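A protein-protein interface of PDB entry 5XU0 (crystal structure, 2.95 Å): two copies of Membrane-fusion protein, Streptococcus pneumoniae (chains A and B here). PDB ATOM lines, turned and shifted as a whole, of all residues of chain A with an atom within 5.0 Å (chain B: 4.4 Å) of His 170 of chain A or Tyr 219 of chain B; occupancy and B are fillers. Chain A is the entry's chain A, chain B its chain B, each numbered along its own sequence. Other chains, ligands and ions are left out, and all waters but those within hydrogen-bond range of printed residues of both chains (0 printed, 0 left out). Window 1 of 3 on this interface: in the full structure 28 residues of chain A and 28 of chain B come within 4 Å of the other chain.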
ATOM      1  N   GLU A  14      -8.703  25.209  33.140  1.00  0.00           N
ATOM      2  CA  GLU A  14      -9.985  24.634  32.775  1.00  0.00           C
ATOM      3  C   GLU A  14     -11.080  25.262  33.624  1.00  0.00           C
ATOM      4  O   GLU A  14     -10.818  25.950  34.615  1.00  0.00           O
ATOM      5  CB  GLU A  14     -10.021  23.115  32.984  1.00  0.00           C
ATOM      6  CG  GLU A  14      -9.049  22.309  32.152  1.00  0.00           C
ATOM      7  CD  GLU A  14      -9.046  20.848  32.561  1.00  0.00           C
ATOM      8  OE1 GLU A  14      -9.334  20.568  33.745  1.00  0.00           O
ATOM      9  OE2 GLU A  14      -8.769  19.983  31.703  1.00  0.00           O
ATOM     10  N   GLN A  15     -12.319  25.005  33.214  1.00  0.00           N
ATOM     11  CA  GLN A  15     -13.494  25.200  34.046  1.00  0.00           C
ATOM     12  C   GLN A  15     -14.525  24.160  33.644  1.00  0.00           C
ATOM     13  O   GLN A  15     -14.881  24.057  32.466  1.00  0.00           O
ATOM     14  CB  GLN A  15     -14.087  26.606  33.910  1.00  0.00           C
ATOM     15  CG  GLN A  15     -15.493  26.715  34.494  1.00  0.00           C
ATOM     16  CD  GLN A  15     -16.189  28.004  34.118  1.00  0.00           C
ATOM     17  OE1 GLN A  15     -15.546  29.031  33.919  1.00  0.00           O
ATOM     18  NE2 GLN A  15     -17.512  27.960  34.025  1.00  0.00           N
ATOM     19  N   TYR A  16     -14.965  23.373  34.614  1.00  0.00           N
ATOM     20  CA  TYR A  16     -16.093  22.476  34.445  1.00  0.00           C
ATOM     21  C   TYR A  16     -17.340  23.139  35.016  1.00  0.00           C
ATOM     22  O   TYR A  16     -17.265  24.016  35.879  1.00  0.00           O
ATOM     23  CB  TYR A  16     -15.842  21.134  35.138  1.00  0.00           C
ATOM     24  CG  TYR A  16     -14.782  20.274  34.482  1.00  0.00           C
ATOM     25  CD1 TYR A  16     -15.130  19.131  33.773  1.00  0.00           C
ATOM     26  CD2 TYR A  16     -13.434  20.596  34.583  1.00  0.00           C
ATOM     27  CE1 TYR A  16     -14.165  18.338  33.177  1.00  0.00           C
ATOM     28  CE2 TYR A  16     -12.463  19.811  33.990  1.00  0.00           C
ATOM     29  CZ  TYR A  16     -12.834  18.682  33.290  1.00  0.00           C
ATOM     30  OH  TYR A  16     -11.868  17.900  32.699  1.00  0.00           O
ATOM     31  N   THR A 149     -11.823  27.644  25.044  1.00  0.00           N
ATOM     32  CA  THR A 149     -12.640  26.940  24.064  1.00  0.00           C
ATOM     33  C   THR A 149     -13.580  26.017  24.813  1.00  0.00           C
ATOM     34  O   THR A 149     -13.123  25.197  25.619  1.00  0.00           O
ATOM     35  CB  THR A 149     -11.779  26.115  23.107  1.00  0.00           C
ATOM     36  OG1 THR A 149     -10.566  26.817  22.826  1.00  0.00           O
ATOM     37  CG2 THR A 149     -12.498  25.921  21.811  1.00  0.00           C
ATOM     38  N   VAL A 150     -14.882  26.161  24.571  1.00  0.00           N
ATOM     39  CA  VAL A 150     -15.818  25.165  25.078  1.00  0.00           C
ATOM     40  C   VAL A 150     -15.663  23.890  24.263  1.00  0.00           C
ATOM     41  O   VAL A 150     -15.723  23.906  23.027  1.00  0.00           O
ATOM     42  CB  VAL A 150     -17.264  25.684  25.044  1.00  0.00           C
ATOM     43  CG1 VAL A 150     -17.581  26.297  23.705  1.00  0.00           C
ATOM     44  CG2 VAL A 150     -18.249  24.558  25.358  1.00  0.00           C
ATOM     45  N   VAL A 151     -15.431  22.777  24.955  1.00  0.00           N
ATOM     46  CA  VAL A 151     -15.170  21.494  24.320  1.00  0.00           C
ATOM     47  C   VAL A 151     -16.256  20.474  24.599  1.00  0.00           C
ATOM     48  O   VAL A 151     -16.172  19.348  24.092  1.00  0.00           O
ATOM     49  CB  VAL A 151     -13.801  20.931  24.743  1.00  0.00           C
ATOM     50  CG1 VAL A 151     -12.714  21.975  24.550  1.00  0.00           C
ATOM     51  CG2 VAL A 151     -13.849  20.460  26.190  1.00  0.00           C
ATOM     52  N   GLU A 152     -17.271  20.821  25.388  1.00  0.00           N
ATOM     53  CA  GLU A 152     -18.303  19.855  25.740  1.00  0.00           C
ATOM     54  C   GLU A 152     -19.532  20.571  26.278  1.00  0.00           C
ATOM     55  O   GLU A 152     -19.426  21.373  27.214  1.00  0.00           O
ATOM     56  CB  GLU A 152     -17.786  18.856  26.780  1.00  0.00           C
ATOM     57  CG  GLU A 152     -18.786  17.778  27.141  1.00  0.00           C
ATOM     58  CD  GLU A 152     -18.234  16.786  28.141  1.00  0.00           C
ATOM     59  OE1 GLU A 152     -17.029  16.873  28.471  1.00  0.00           O
ATOM     60  OE2 GLU A 152     -19.008  15.920  28.600  1.00  0.00           O
ATOM     61  N   VAL A 167     -21.372  16.433  33.895  1.00  0.00           N
ATOM     62  CA  VAL A 167     -20.769  17.607  33.280  1.00  0.00           C
ATOM     63  C   VAL A 167     -21.760  18.233  32.307  1.00  0.00           C
ATOM     64  O   VAL A 167     -22.473  17.534  31.576  1.00  0.00           O
ATOM     65  CB  VAL A 167     -19.451  17.218  32.586  1.00  0.00           C
ATOM     66  CG1 VAL A 167     -19.658  15.992  31.707  1.00  0.00           C
ATOM     67  CG2 VAL A 167     -18.896  18.379  31.774  1.00  0.00           C
ATOM     68  N   MET A 168     -21.826  19.561  32.311  1.00  0.00           N
ATOM     69  CA  MET A 168     -22.750  20.281  31.441  1.00  0.00           C
ATOM     70  C   MET A 168     -22.007  21.153  30.442  1.00  0.00           C
ATOM     71  O   MET A 168     -22.397  21.248  29.281  1.00  0.00           O
ATOM     72  CB  MET A 168     -23.708  21.142  32.265  1.00  0.00           C
ATOM     73  CG  MET A 168     -24.864  20.377  32.877  1.00  0.00           C
ATOM     74  SD  MET A 168     -26.300  21.583  33.402  1.00  0.00           S
ATOM     75  CE  MET A 168     -25.209  23.119  33.891  1.00  0.00           C
ATOM     76  N   VAL A 169     -20.943  21.802  30.903  1.00  0.00           N
ATOM     77  CA  VAL A 169     -20.078  22.599  30.039  1.00  0.00           C
ATOM     78  C   VAL A 169     -18.641  22.379  30.479  1.00  0.00           C
ATOM     79  O   VAL A 169     -18.340  22.429  31.676  1.00  0.00           O
ATOM     80  CB  VAL A 169     -20.422  24.101  30.089  1.00  0.00           C
ATOM     81  CG1 VAL A 169     -19.211  24.925  29.697  1.00  0.00           C
ATOM     82  CG2 VAL A 169     -21.583  24.409  29.176  1.00  0.00           C
ATOM     83  N   HIS A 170     -17.752  22.133  29.521  1.00  0.00           N
ATOM     84  CA  HIS A 170     -16.325  22.063  29.799  1.00  0.00           C
ATOM     85  C   HIS A 170     -15.593  23.063  28.916  1.00  0.00           C
ATOM     86  O   HIS A 170     -15.679  22.994  27.684  1.00  0.00           O
ATOM     87  CB  HIS A 170     -15.776  20.655  29.582  1.00  0.00           C
ATOM     88  CG  HIS A 170     -14.358  20.496  30.034  1.00  0.00           C
ATOM     89  ND1 HIS A 170     -13.562  19.440  29.642  1.00  0.00           N
ATOM     90  CD2 HIS A 170     -13.591  21.264  30.843  1.00  0.00           C
ATOM     91  CE1 HIS A 170     -12.367  19.566  30.190  1.00  0.00           C
ATOM     92  NE2 HIS A 170     -12.359  20.664  30.924  1.00  0.00           N
ATOM     93  N   ILE A 171     -14.872  23.981  29.549  1.00  0.00           N
ATOM     94  CA  ILE A 171     -14.072  24.991  28.864  1.00  0.00           C
ATOM     95  C   ILE A 171     -12.614  24.760  29.232  1.00  0.00           C
ATOM     96  O   ILE A 171     -12.299  24.552  30.410  1.00  0.00           O
ATOM     97  CB  ILE A 171     -14.515  26.410  29.259  1.00  0.00           C
ATOM     98  CG1 ILE A 171     -15.865  26.730  28.640  1.00  0.00           C
ATOM     99  CG2 ILE A 171     -13.470  27.443  28.847  1.00  0.00           C
ATOM    100  CD1 ILE A 171     -16.254  28.137  28.835  1.00  0.00           C
ATOM    101  N   VAL A 172     -11.727  24.777  28.233  1.00  0.00           N
ATOM    102  CA  VAL A 172     -10.293  24.753  28.491  1.00  0.00           C
ATOM    103  C   VAL A 172      -9.635  25.837  27.650  1.00  0.00           C
ATOM    104  O   VAL A 172     -10.014  26.062  26.496  1.00  0.00           O
ATOM    105  CB  VAL A 172      -9.660  23.364  28.225  1.00  0.00           C
ATOM    106  CG1 VAL A 172     -10.538  22.245  28.774  1.00  0.00           C
ATOM    107  CG2 VAL A 172      -9.384  23.148  26.753  1.00  0.00           C
ATOM    108  N   GLN A 254      -2.959  20.692  21.937  1.00  0.00           N
ATOM    109  CA  GLN A 254      -3.031  19.941  23.179  1.00  0.00           C
ATOM    110  C   GLN A 254      -2.989  18.447  22.879  1.00  0.00           C
ATOM    111  O   GLN A 254      -3.350  18.002  21.787  1.00  0.00           O
ATOM    112  CB  GLN A 254      -4.311  20.303  23.933  1.00  0.00           C
ATOM    113  CG  GLN A 254      -4.345  21.737  24.443  1.00  0.00           C
ATOM    114  CD  GLN A 254      -5.709  22.126  24.987  1.00  0.00           C
ATOM    115  OE1 GLN A 254      -6.492  21.270  25.396  1.00  0.00           O
ATOM    116  NE2 GLN A 254      -5.998  23.423  24.995  1.00  0.00           N
ATOM    117  N   SER B 217     -11.820  18.771  16.967  1.00  0.00           N
ATOM    118  CA  SER B 217     -11.585  19.166  18.351  1.00  0.00           C
ATOM    119  C   SER B 217     -10.105  19.431  18.602  1.00  0.00           C
ATOM    120  O   SER B 217      -9.258  18.561  18.367  1.00  0.00           O
ATOM    121  CB  SER B 217     -12.093  18.095  19.309  1.00  0.00           C
ATOM    122  OG  SER B 217     -11.900  18.494  20.657  1.00  0.00           O
ATOM    123  N   ASP B 218      -9.804  20.638  19.089  1.00  0.00           N
ATOM    124  CA  ASP B 218      -8.491  20.965  19.636  1.00  0.00           C
ATOM    125  C   ASP B 218      -8.142  20.132  20.858  1.00  0.00           C
ATOM    126  O   ASP B 218      -6.956  20.003  21.179  1.00  0.00           O
ATOM    127  CB  ASP B 218      -8.429  22.446  20.023  1.00  0.00           C
ATOM    128  CG  ASP B 218      -7.798  23.306  18.954  1.00  0.00           C
ATOM    129  OD1 ASP B 218      -7.679  22.848  17.797  1.00  0.00           O
ATOM    130  OD2 ASP B 218      -7.423  24.455  19.279  1.00  0.00           O
ATOM    131  N   TYR B 219      -9.137  19.563  21.533  1.00  0.00           N
ATOM    132  CA  TYR B 219      -8.950  19.003  22.859  1.00  0.00           C
ATOM    133  C   TYR B 219      -8.991  17.487  22.791  1.00  0.00           C
ATOM    134  O   TYR B 219      -9.991  16.927  22.318  1.00  0.00           O
ATOM    135  CB  TYR B 219     -10.032  19.523  23.797  1.00  0.00           C
ATOM    136  CG  TYR B 219      -9.971  18.967  25.192  1.00  0.00           C
ATOM    137  CD1 TYR B 219     -10.840  17.964  25.596  1.00  0.00           C
ATOM    138  CD2 TYR B 219      -9.048  19.449  26.111  1.00  0.00           C
ATOM    139  CE1 TYR B 219     -10.791  17.452  26.877  1.00  0.00           C
ATOM    140  CE2 TYR B 219      -8.990  18.942  27.395  1.00  0.00           C
ATOM    141  CZ  TYR B 219      -9.864  17.945  27.772  1.00  0.00           C
ATOM    142  OH  TYR B 219      -9.816  17.431  29.047  1.00  0.00           O
ATOM    143  N   PRO B 220      -7.956  16.784  23.248  1.00  0.00           N
ATOM    144  CA  PRO B 220      -7.958  15.321  23.148  1.00  0.00           C
ATOM    145  C   PRO B 220      -8.929  14.688  24.131  1.00  0.00           C
ATOM    146  O   PRO B 220      -9.133  15.181  25.243  1.00  0.00           O
ATOM    147  CB  PRO B 220      -6.511  14.946  23.483  1.00  0.00           C
ATOM    148  CG  PRO B 220      -6.051  16.044  24.391  1.00  0.00           C
ATOM    149  CD  PRO B 220      -6.759  17.299  23.939  1.00  0.00           C
ATOM    150  N   LYS B 221      -9.540  13.584  23.699  1.00  0.00           N
ATOM    151  CA  LYS B 221     -10.357  12.773  24.594  1.00  0.00           C
ATOM    152  C   LYS B 221      -9.497  12.325  25.772  1.00  0.00           C
ATOM    153  O   LYS B 221      -8.360  11.880  25.585  1.00  0.00           O
ATOM    154  CB  LYS B 221     -10.944  11.577  23.821  1.00  0.00           C
ATOM    155  CG  LYS B 221     -11.907  10.612  24.555  1.00  0.00           C
ATOM    156  CD  LYS B 221     -12.481   9.479  23.700  1.00  0.00           C
ATOM    157  CE  LYS B 221     -13.392   8.589  24.546  1.00  0.00           C
ATOM    158  NZ  LYS B 221     -13.985   7.465  23.774  1.00  0.00           N
ATOM    159  N   TYR B 239      -8.371  12.823  18.824  1.00  0.00           N
ATOM    160  CA  TYR B 239      -9.208  14.015  18.865  1.00  0.00           C
ATOM    161  C   TYR B 239     -10.507  13.781  18.113  1.00  0.00           C
ATOM    162  O   TYR B 239     -10.464  13.389  16.942  1.00  0.00           O
ATOM    163  CB  TYR B 239      -8.469  15.207  18.250  1.00  0.00           C
ATOM    164  CG  TYR B 239      -7.095  15.440  18.827  1.00  0.00           C
ATOM    165  CD1 TYR B 239      -6.902  16.354  19.852  1.00  0.00           C
ATOM    166  CD2 TYR B 239      -5.991  14.747  18.349  1.00  0.00           C
ATOM    167  CE1 TYR B 239      -5.650  16.570  20.384  1.00  0.00           C
ATOM    168  CE2 TYR B 239      -4.734  14.955  18.879  1.00  0.00           C
ATOM    169  CZ  TYR B 239      -4.569  15.869  19.894  1.00  0.00           C
ATOM    170  OH  TYR B 239      -3.318  16.084  20.425  1.00  0.00           O
ATOM    171  N   PRO B 240     -11.667  14.031  18.713  1.00  0.00           N
ATOM    172  CA  PRO B 240     -12.928  13.733  18.020  1.00  0.00           C
ATOM    173  C   PRO B 240     -13.212  14.701  16.878  1.00  0.00           C
ATOM    174  O   PRO B 240     -12.931  15.898  16.962  1.00  0.00           O
ATOM    175  CB  PRO B 240     -13.976  13.864  19.131  1.00  0.00           C
ATOM    176  CG  PRO B 240     -13.377  14.819  20.098  1.00  0.00           C
ATOM    177  CD  PRO B 240     -11.889  14.594  20.057  1.00  0.00           C
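The backbone carbonyl oxygen (O) of Gln 254 of chain A lies close to the side-chain hydroxyl (OH) of Tyr 239 of chain B.
The backbone carbonyl oxygen (O) of Glu 152 of chain A lies within hydrogen-bond range of the backbone NH (N) of His 170 of chain A. The backbone NH of Thr 149 of chain A lies within hydrogen-bond range of the backbone carbonyl oxygen of Val 172 of chain A, 2.8 Å away. N of Val 151 of chain A lies within hydrogen-bond range of O of His 170 of chain A. The side-chain hydroxyl (OH) of Tyr 16 of chain A lies close to a ring nitrogen (NE2) of His 170 of chain A (3.3 Å). The side-chain hydroxyl (OG) of Ser 217 of chain B lies within hydrogen-bond range of the backbone carbonyl oxygen (O) of Tyr 219 of chain B.
Glu 14 of chain A touches Tyr 219 of chain B (OE2 to OH, 3.8 Å). Val 151 of chain A touches Tyr 219 of chain B. His 170 of chain A touches Tyr 219 of chain B. CG2 of Val 172 of chain A touches CD2 of Tyr 219 of chain B (3.8 Å). Asp 218 of chain B touches Gln 254 of chain A. OE1 of Gln 254 of chain A touches CD2 of Tyr 219 of chain B (3.2 Å). CD of Pro 220 of chain B touches CB of Gln 254 of chain A, 3.9 Å away.
Of chain B, only Tyr 219 (3.5 Å) comes within 4 Å of His 170 of chain A. Tyr 219 of chain B touches five residues of chain A. Of the printed residues of chain B, Gln 254 of chain A touches Asp 218 (3.8 Å), Tyr 219 (3.2 Å), Pro 220 (3.9 Å) and Tyr 239 (2.4 Å). Of the printed residues of chain B, Val 172 of chain A touches Tyr 219. Thr 149 of chain A touches none of the printed residues of chain B. Met 168 of chain A touches none of the printed residues of chain B. The nearest printed residue of chain B that does not touch His 170 of chain A is Pro 220 of chain B (7.4 Å). The nearest residue of chain A that does not touch Tyr 219 of chain B is Tyr 16 of chain A (4.2 Å).
Of the 14 printed residues of chain A, 5 touch a printed residue of chain B. Printed residues of chain A that touch a printed residue of chain B: Glu 14, Val 151, His 170, Val 172 and Gln 254. Of the 7 printed residues of chain B, 4 touch a printed residue of chain A. Printed residues of chain B that touch a printed residue of chain A: Asp 218, Tyr 219, Pro 220 and Tyr 239.
No position is printed for both chains. Of the 8 pairs that touch across the chains among the printed residues, none has its exchanged pair printed and touching as well.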
